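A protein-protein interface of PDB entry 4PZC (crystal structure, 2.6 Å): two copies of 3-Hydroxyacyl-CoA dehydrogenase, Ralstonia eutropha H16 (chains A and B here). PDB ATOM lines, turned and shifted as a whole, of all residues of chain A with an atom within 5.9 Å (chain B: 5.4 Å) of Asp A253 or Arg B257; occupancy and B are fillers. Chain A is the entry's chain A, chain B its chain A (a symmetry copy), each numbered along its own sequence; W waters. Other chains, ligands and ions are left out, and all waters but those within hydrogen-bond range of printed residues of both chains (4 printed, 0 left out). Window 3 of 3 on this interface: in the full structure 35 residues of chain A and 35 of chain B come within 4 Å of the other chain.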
ATOM      1  N   LEU A 247       0.868  22.090 -34.850  1.00  0.00           N
ATOM      2  CA  LEU A 247       0.469  22.095 -33.466  1.00  0.00           C
ATOM      3  C   LEU A 247      -1.047  22.327 -33.322  1.00  0.00           C
ATOM      4  O   LEU A 247      -1.714  21.541 -32.645  1.00  0.00           O
ATOM      5  CB  LEU A 247       1.268  23.120 -32.699  1.00  0.00           C
ATOM      6  CG  LEU A 247       2.767  22.819 -32.549  1.00  0.00           C
ATOM      7  CD1 LEU A 247       3.415  23.921 -31.722  1.00  0.00           C
ATOM      8  CD2 LEU A 247       3.074  21.490 -31.893  1.00  0.00           C
ATOM      9  N   TYR A 248      -1.582  23.377 -33.960  1.00  0.00           N
ATOM     10  CA  TYR A 248      -3.044  23.661 -33.947  1.00  0.00           C
ATOM     11  C   TYR A 248      -3.854  22.483 -34.495  1.00  0.00           C
ATOM     12  O   TYR A 248      -4.892  22.102 -33.960  1.00  0.00           O
ATOM     13  CB  TYR A 248      -3.377  24.978 -34.728  1.00  0.00           C
ATOM     14  CG  TYR A 248      -4.872  25.278 -34.905  1.00  0.00           C
ATOM     15  CD1 TYR A 248      -5.705  25.420 -33.805  1.00  0.00           C
ATOM     16  CD2 TYR A 248      -5.444  25.413 -36.175  1.00  0.00           C
ATOM     17  CE1 TYR A 248      -7.073  25.669 -33.953  1.00  0.00           C
ATOM     18  CE2 TYR A 248      -6.811  25.669 -36.329  1.00  0.00           C
ATOM     19  CZ  TYR A 248      -7.630  25.792 -35.219  1.00  0.00           C
ATOM     20  OH  TYR A 248      -8.986  26.048 -35.363  1.00  0.00           O
ATOM     21  N   THR A 249      -3.364  21.886 -35.553  1.00  0.00           N
ATOM     22  CA  THR A 249      -4.127  20.861 -36.216  1.00  0.00           C
ATOM     23  C   THR A 249      -4.059  19.553 -35.456  1.00  0.00           C
ATOM     24  O   THR A 249      -5.068  18.907 -35.316  1.00  0.00           O
ATOM     25  CB  THR A 249      -3.679  20.698 -37.682  1.00  0.00           C
ATOM     26  OG1 THR A 249      -3.751  21.973 -38.310  1.00  0.00           O
ATOM     27  CG2 THR A 249      -4.611  19.760 -38.437  1.00  0.00           C
ATOM     28  N   PHE A 251      -3.007  19.008 -32.102  1.00  0.00           N
ATOM     29  CA  PHE A 251      -3.634  19.236 -30.791  1.00  0.00           C
ATOM     30  C   PHE A 251      -5.093  19.642 -30.830  1.00  0.00           C
ATOM     31  O   PHE A 251      -5.802  19.458 -29.807  1.00  0.00           O
ATOM     32  CB  PHE A 251      -2.878  20.277 -29.982  1.00  0.00           C
ATOM     33  CG  PHE A 251      -1.625  19.751 -29.402  1.00  0.00           C
ATOM     34  CD1 PHE A 251      -1.656  18.617 -28.602  1.00  0.00           C
ATOM     35  CD2 PHE A 251      -0.402  20.367 -29.664  1.00  0.00           C
ATOM     36  CE1 PHE A 251      -0.489  18.109 -28.074  1.00  0.00           C
ATOM     37  CE2 PHE A 251       0.774  19.869 -29.138  1.00  0.00           C
ATOM     38  CZ  PHE A 251       0.731  18.730 -28.343  1.00  0.00           C
ATOM     39  N   ALA A 252      -5.515  20.173 -31.987  1.00  0.00           N
ATOM     40  CA  ALA A 252      -6.872  20.687 -32.183  1.00  0.00           C
ATOM     41  C   ALA A 252      -7.202  21.731 -31.148  1.00  0.00           C
ATOM     42  O   ALA A 252      -8.272  21.666 -30.547  1.00  0.00           O
ATOM     43  CB  ALA A 252      -7.909  19.569 -32.144  1.00  0.00           C
ATOM     44  N   ASP A 253      -6.294  22.698 -30.965  1.00  0.00           N
ATOM     45  CA  ASP A 253      -6.365  23.674 -29.862  1.00  0.00           C
ATOM     46  C   ASP A 253      -5.840  25.068 -30.299  1.00  0.00           C
ATOM     47  O   ASP A 253      -4.656  25.212 -30.602  1.00  0.00           O
ATOM     48  CB  ASP A 253      -5.572  23.102 -28.682  1.00  0.00           C
ATOM     49  CG  ASP A 253      -5.666  23.920 -27.405  1.00  0.00           C
ATOM     50  OD1 ASP A 253      -6.324  24.990 -27.286  1.00  0.00           O
ATOM     51  OD2 ASP A 253      -5.020  23.424 -26.469  1.00  0.00           O
ATOM     52  N   PRO A 254      -6.736  26.087 -30.354  1.00  0.00           N
ATOM     53  CA  PRO A 254      -6.376  27.457 -30.739  1.00  0.00           C
ATOM     54  C   PRO A 254      -5.308  28.078 -29.886  1.00  0.00           C
ATOM     55  O   PRO A 254      -4.772  29.127 -30.263  1.00  0.00           O
ATOM     56  CB  PRO A 254      -7.683  28.254 -30.568  1.00  0.00           C
ATOM     57  CG  PRO A 254      -8.574  27.369 -29.755  1.00  0.00           C
ATOM     58  CD  PRO A 254      -8.190  25.969 -30.168  1.00  0.00           C
ATOM     59  N   LYS A 255      -4.995  27.474 -28.751  1.00  0.00           N
ATOM     60  CA  LYS A 255      -3.852  27.934 -27.975  1.00  0.00           C
ATOM     61  C   LYS A 255      -2.666  28.141 -28.899  1.00  0.00           C
ATOM     62  O   LYS A 255      -1.867  29.038 -28.705  1.00  0.00           O
ATOM     63  CB  LYS A 255      -3.489  26.922 -26.872  1.00  0.00           C
ATOM     64  CG  LYS A 255      -2.100  27.124 -26.277  1.00  0.00           C
ATOM     65  CD  LYS A 255      -1.923  26.413 -24.940  1.00  0.00           C
ATOM     66  CE  LYS A 255      -0.467  26.529 -24.523  1.00  0.00           C
ATOM     67  NZ  LYS A 255      -0.040  25.708 -23.368  1.00  0.00           N
ATOM     68  N   TYR A 256      -2.567  27.281 -29.903  1.00  0.00           N
ATOM     69  CA  TYR A 256      -1.454  27.299 -30.854  1.00  0.00           C
ATOM     70  C   TYR A 256      -1.755  27.971 -32.201  1.00  0.00           C
ATOM     71  O   TYR A 256      -0.987  27.786 -33.123  1.00  0.00           O
ATOM     72  CB  TYR A 256      -0.988  25.845 -31.087  1.00  0.00           C
ATOM     73  CG  TYR A 256      -0.705  25.121 -29.788  1.00  0.00           C
ATOM     74  CD1 TYR A 256      -1.702  24.417 -29.116  1.00  0.00           C
ATOM     75  CD2 TYR A 256       0.566  25.178 -29.216  1.00  0.00           C
ATOM     76  CE1 TYR A 256      -1.432  23.773 -27.909  1.00  0.00           C
ATOM     77  CE2 TYR A 256       0.854  24.559 -28.015  1.00  0.00           C
ATOM     78  CZ  TYR A 256      -0.137  23.857 -27.367  1.00  0.00           C
ATOM     79  OH  TYR A 256       0.198  23.264 -26.188  1.00  0.00           O
ATOM     80  N   ARG A 257      -2.870  28.707 -32.319  1.00  0.00           N
ATOM     81  CA  ARG A 257      -3.136  29.628 -33.447  1.00  0.00           C
ATOM     82  C   ARG A 257      -1.870  30.223 -34.018  1.00  0.00           C
ATOM     83  O   ARG A 257      -1.118  30.865 -33.289  1.00  0.00           O
ATOM     84  CB  ARG A 257      -3.868  30.860 -32.931  1.00  0.00           C
ATOM     85  CG  ARG A 257      -5.376  30.868 -32.984  1.00  0.00           C
ATOM     86  CD  ARG A 257      -5.866  32.137 -32.267  1.00  0.00           C
ATOM     87  NE  ARG A 257      -5.703  32.028 -30.823  1.00  0.00           N
ATOM     88  CZ  ARG A 257      -5.861  33.011 -29.943  1.00  0.00           C
ATOM     89  NH1 ARG A 257      -6.152  34.240 -30.334  1.00  0.00           N
ATOM     90  NH2 ARG A 257      -5.708  32.751 -28.640  1.00  0.00           N
ATOM     91  N   ASN B 198       5.933  28.095 -19.164  1.00  0.00           N
ATOM     92  CA  ASN B 198       4.694  27.338 -19.091  1.00  0.00           C
ATOM     93  C   ASN B 198       4.583  26.119 -20.021  1.00  0.00           C
ATOM     94  O   ASN B 198       4.152  25.015 -19.598  1.00  0.00           O
ATOM     95  CB  ASN B 198       3.519  28.231 -19.422  1.00  0.00           C
ATOM     96  CG  ASN B 198       2.301  27.813 -18.691  1.00  0.00           C
ATOM     97  OD1 ASN B 198       1.221  27.713 -19.257  1.00  0.00           O
ATOM     98  ND2 ASN B 198       2.473  27.562 -17.380  1.00  0.00           N
ATOM     99  N   MET B 244       1.515  34.094 -15.369  1.00  0.00           N
ATOM    100  CA  MET B 244       0.558  33.432 -16.222  1.00  0.00           C
ATOM    101  C   MET B 244      -0.847  33.750 -15.767  1.00  0.00           C
ATOM    102  O   MET B 244      -1.712  33.876 -16.591  1.00  0.00           O
ATOM    103  CB  MET B 244       0.755  31.917 -16.199  1.00  0.00           C
ATOM    104  CG  MET B 244       2.071  31.459 -16.765  1.00  0.00           C
ATOM    105  SD  MET B 244       2.149  31.741 -18.536  1.00  0.00           S
ATOM    106  CE  MET B 244       3.828  32.235 -18.470  1.00  0.00           C
ATOM    107  N   TYR B 248      -3.644  35.241 -18.522  1.00  0.00           N
ATOM    108  CA  TYR B 248      -5.010  34.675 -18.697  1.00  0.00           C
ATOM    109  C   TYR B 248      -6.093  35.664 -18.257  1.00  0.00           C
ATOM    110  O   TYR B 248      -7.119  35.839 -18.909  1.00  0.00           O
ATOM    111  CB  TYR B 248      -5.163  33.309 -17.943  1.00  0.00           C
ATOM    112  CG  TYR B 248      -6.579  32.719 -17.932  1.00  0.00           C
ATOM    113  CD1 TYR B 248      -7.240  32.427 -19.117  1.00  0.00           C
ATOM    114  CD2 TYR B 248      -7.253  32.459 -16.733  1.00  0.00           C
ATOM    115  CE1 TYR B 248      -8.539  31.913 -19.121  1.00  0.00           C
ATOM    116  CE2 TYR B 248      -8.551  31.938 -16.730  1.00  0.00           C
ATOM    117  CZ  TYR B 248      -9.200  31.668 -17.924  1.00  0.00           C
ATOM    118  OH  TYR B 248     -10.486  31.148 -17.930  1.00  0.00           O
ATOM    119  N   ASP B 253      -8.030  35.012 -22.035  1.00  0.00           N
ATOM    120  CA  ASP B 253      -7.784  34.053 -23.129  1.00  0.00           C
ATOM    121  C   ASP B 253      -7.046  32.785 -22.620  1.00  0.00           C
ATOM    122  O   ASP B 253      -5.899  32.874 -22.184  1.00  0.00           O
ATOM    123  CB  ASP B 253      -6.992  34.783 -24.218  1.00  0.00           C
ATOM    124  CG  ASP B 253      -6.779  33.978 -25.488  1.00  0.00           C
ATOM    125  OD1 ASP B 253      -7.195  32.800 -25.668  1.00  0.00           O
ATOM    126  OD2 ASP B 253      -6.141  34.601 -26.351  1.00  0.00           O
ATOM    127  N   PRO B 254      -7.725  31.609 -22.654  1.00  0.00           N
ATOM    128  CA  PRO B 254      -7.148  30.333 -22.216  1.00  0.00           C
ATOM    129  C   PRO B 254      -5.889  29.944 -22.937  1.00  0.00           C
ATOM    130  O   PRO B 254      -5.203  29.016 -22.490  1.00  0.00           O
ATOM    131  CB  PRO B 254      -8.245  29.296 -22.524  1.00  0.00           C
ATOM    132  CG  PRO B 254      -9.195  29.997 -23.441  1.00  0.00           C
ATOM    133  CD  PRO B 254      -9.143  31.440 -23.003  1.00  0.00           C
ATOM    134  N   LYS B 255      -5.576  30.610 -24.036  1.00  0.00           N
ATOM    135  CA  LYS B 255      -4.285  30.393 -24.673  1.00  0.00           C
ATOM    136  C   LYS B 255      -3.193  30.413 -23.620  1.00  0.00           C
ATOM    137  O   LYS B 255      -2.216  29.693 -23.713  1.00  0.00           O
ATOM    138  CB  LYS B 255      -4.007  31.469 -25.740  1.00  0.00           C
ATOM    139  CG  LYS B 255      -2.548  31.551 -26.173  1.00  0.00           C
ATOM    140  CD  LYS B 255      -2.365  32.298 -27.489  1.00  0.00           C
ATOM    141  CE  LYS B 255      -0.877  32.476 -27.739  1.00  0.00           C
ATOM    142  NZ  LYS B 255      -0.493  33.377 -28.848  1.00  0.00           N
ATOM    143  N   TYR B 256      -3.378  31.264 -22.621  1.00  0.00           N
ATOM    144  CA  TYR B 256      -2.397  31.456 -21.551  1.00  0.00           C
ATOM    145  C   TYR B 256      -2.710  30.723 -20.238  1.00  0.00           C
ATOM    146  O   TYR B 256      -2.102  31.045 -19.238  1.00  0.00           O
ATOM    147  CB  TYR B 256      -2.257  32.970 -21.283  1.00  0.00           C
ATOM    148  CG  TYR B 256      -1.978  33.751 -22.551  1.00  0.00           C
ATOM    149  CD1 TYR B 256      -3.012  34.251 -23.337  1.00  0.00           C
ATOM    150  CD2 TYR B 256      -0.664  33.951 -22.975  1.00  0.00           C
ATOM    151  CE1 TYR B 256      -2.741  34.949 -24.514  1.00  0.00           C
ATOM    152  CE2 TYR B 256      -0.371  34.628 -24.143  1.00  0.00           C
ATOM    153  CZ  TYR B 256      -1.401  35.129 -24.906  1.00  0.00           C
ATOM    154  OH  TYR B 256      -1.059  35.789 -26.046  1.00  0.00           O
ATOM    155  N   ARG B 257      -3.664  29.780 -20.238  1.00  0.00           N
ATOM    156  CA  ARG B 257      -3.868  28.812 -19.137  1.00  0.00           C
ATOM    157  C   ARG B 257      -2.583  28.471 -18.421  1.00  0.00           C
ATOM    158  O   ARG B 257      -1.642  27.998 -19.054  1.00  0.00           O
ATOM    159  CB  ARG B 257      -4.281  27.466 -19.718  1.00  0.00           C
ATOM    160  CG  ARG B 257      -5.754  27.161 -19.835  1.00  0.00           C
ATOM    161  CD  ARG B 257      -5.901  25.828 -20.588  1.00  0.00           C
ATOM    162  NE  ARG B 257      -5.601  25.983 -22.006  1.00  0.00           N
ATOM    163  CZ  ARG B 257      -5.463  24.999 -22.887  1.00  0.00           C
ATOM    164  NH1 ARG B 257      -5.548  23.732 -22.518  1.00  0.00           N
ATOM    165  NH2 ARG B 257      -5.219  25.298 -24.167  1.00  0.00           N
ATOM    166  N   PRO B 258      -2.522  28.668 -17.112  1.00  0.00           N
ATOM    167  CA  PRO B 258      -1.374  28.045 -16.427  1.00  0.00           C
ATOM    168  C   PRO B 258      -1.278  26.519 -16.582  1.00  0.00           C
ATOM    169  O   PRO B 258      -2.309  25.810 -16.599  1.00  0.00           O
ATOM    170  CB  PRO B 258      -1.588  28.412 -14.932  1.00  0.00           C
ATOM    171  CG  PRO B 258      -2.727  29.361 -14.926  1.00  0.00           C
ATOM    172  CD  PRO B 258      -3.057  29.779 -16.335  1.00  0.00           C
ATOM    173  N   ALA B 259      -0.039  26.030 -16.650  1.00  0.00           N
ATOM    174  CA  ALA B 259       0.238  24.581 -16.692  1.00  0.00           C
ATOM    175  C   ALA B 259      -0.164  23.951 -15.371  1.00  0.00           C
ATOM    176  O   ALA B 259       0.246  24.443 -14.318  1.00  0.00           O
ATOM    177  CB  ALA B 259       1.715  24.314 -16.973  1.00  0.00           C
HETATM  178  O   HOH W   1      -8.249  25.918 -25.250  1.00  0.00           O
HETATM  179  O   HOH W   2      -0.901  30.780 -30.408  1.00  0.00           O
HETATM  180  O   HOH W   3      -8.658  31.534 -27.898  1.00  0.00           O
HETATM  181  O   HOH W   4      -1.124  28.156 -21.892  1.00  0.00           O
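CD of Lys A255 touches O of Lys B255 (3.5 Å). Arg B257 touches Lys A255. CD of Lys B255 touches NH2 of Arg A257 (3.6 Å).
The backbone carbonyl oxygen (O) of Tyr A248 lies within hydrogen-bond range of the backbone NH (N) of Asp A253 (3.4 Å). OD1 of Asp A253 sits close to N of Lys A255 (3.2 Å). The backbone carbonyl oxygen (O) of Pro A254 is in hydrogen-bond range of the guanidinium group (NE) of Arg A257. OD1 of Asn B198 lies close to O of Arg B257. O of Tyr B248 sits at hydrogen-bond distance from N of Asp B253, 3.4 Å away. The backbone NH of Lys B255 sits close to the side-chain carboxylate of Asp B253, at 3.2 Å.
The side-chain carboxylate of Asp A253 is in salt-bridge range of the guanidinium group of Arg B257 (3.0 Å). NH2 of Arg A257 lies within salt-bridge range of OD2 of Asp B253, 3.0 Å away.
Water W2 lies within hydrogen-bond range of O of Lys A255, O of Arg A257 and NZ of Lys B255. Water W4 lies within hydrogen-bond range of O of Lys B255 (2.6 Å), O of Arg B257 (2.9 Å) and NZ of Lys A255 (3.1 Å). Water W3 lies within hydrogen-bond range of the side-chain carboxylate (OD1) of Asp B253 and the guanidinium group (NH2) of Arg A257. Water W1 lies within hydrogen-bond range of the side-chain carboxylate of Asp A253 (3.0 Å) and the guanidinium group of Arg B257 (3.3 Å).
Asp A253 touches one residue of chain B. Of the printed residues of chain A, Asp B253 touches Arg A257 (3.0 Å). Printed residues of chain B within 4 Å of Arg A257: Asp B253 (3.0 Å) and Lys B255 (3.6 Å). Printed residues of chain A within 4 Å of Lys B255: Lys A255 (3.5 Å) and Arg A257 (3.6 Å). Printed residues of chain B within 4 Å of Lys A255: Lys B255 and Arg B257. Tyr A256 touches none of the printed residues of chain B. The nearest residue of chain A that does not touch Arg B257 is Tyr A256 (5.5 Å). The nearest printed residue of chain A that does not touch Lys B255 is Pro A254 (4.9 Å).
Asp A253 touches Arg B257, and with the chains exchanged Arg A257 touches Asp B253. Lys A255 touches its own counterpart, Lys B255. Lys A255 touches Arg B257, and with the chains exchanged Arg A257 touches Lys B255. 6 positions are printed for both chains. Of the 5 pairs that touch across the chains among the printed residues, 5 have their exchanged pair printed and touching as well.
Of the 10 printed residues of chain B, 3 touch a printed residue of chain A. Of the 10 printed residues of chain A, 3 touch a printed residue of chain B. Among the printed residues, Asp or Glu carboxylates within 4 Å of a Lys or Arg side-chain nitrogen of the other chain: Asp A253 with Arg B257 and Arg A257 with Asp B253.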
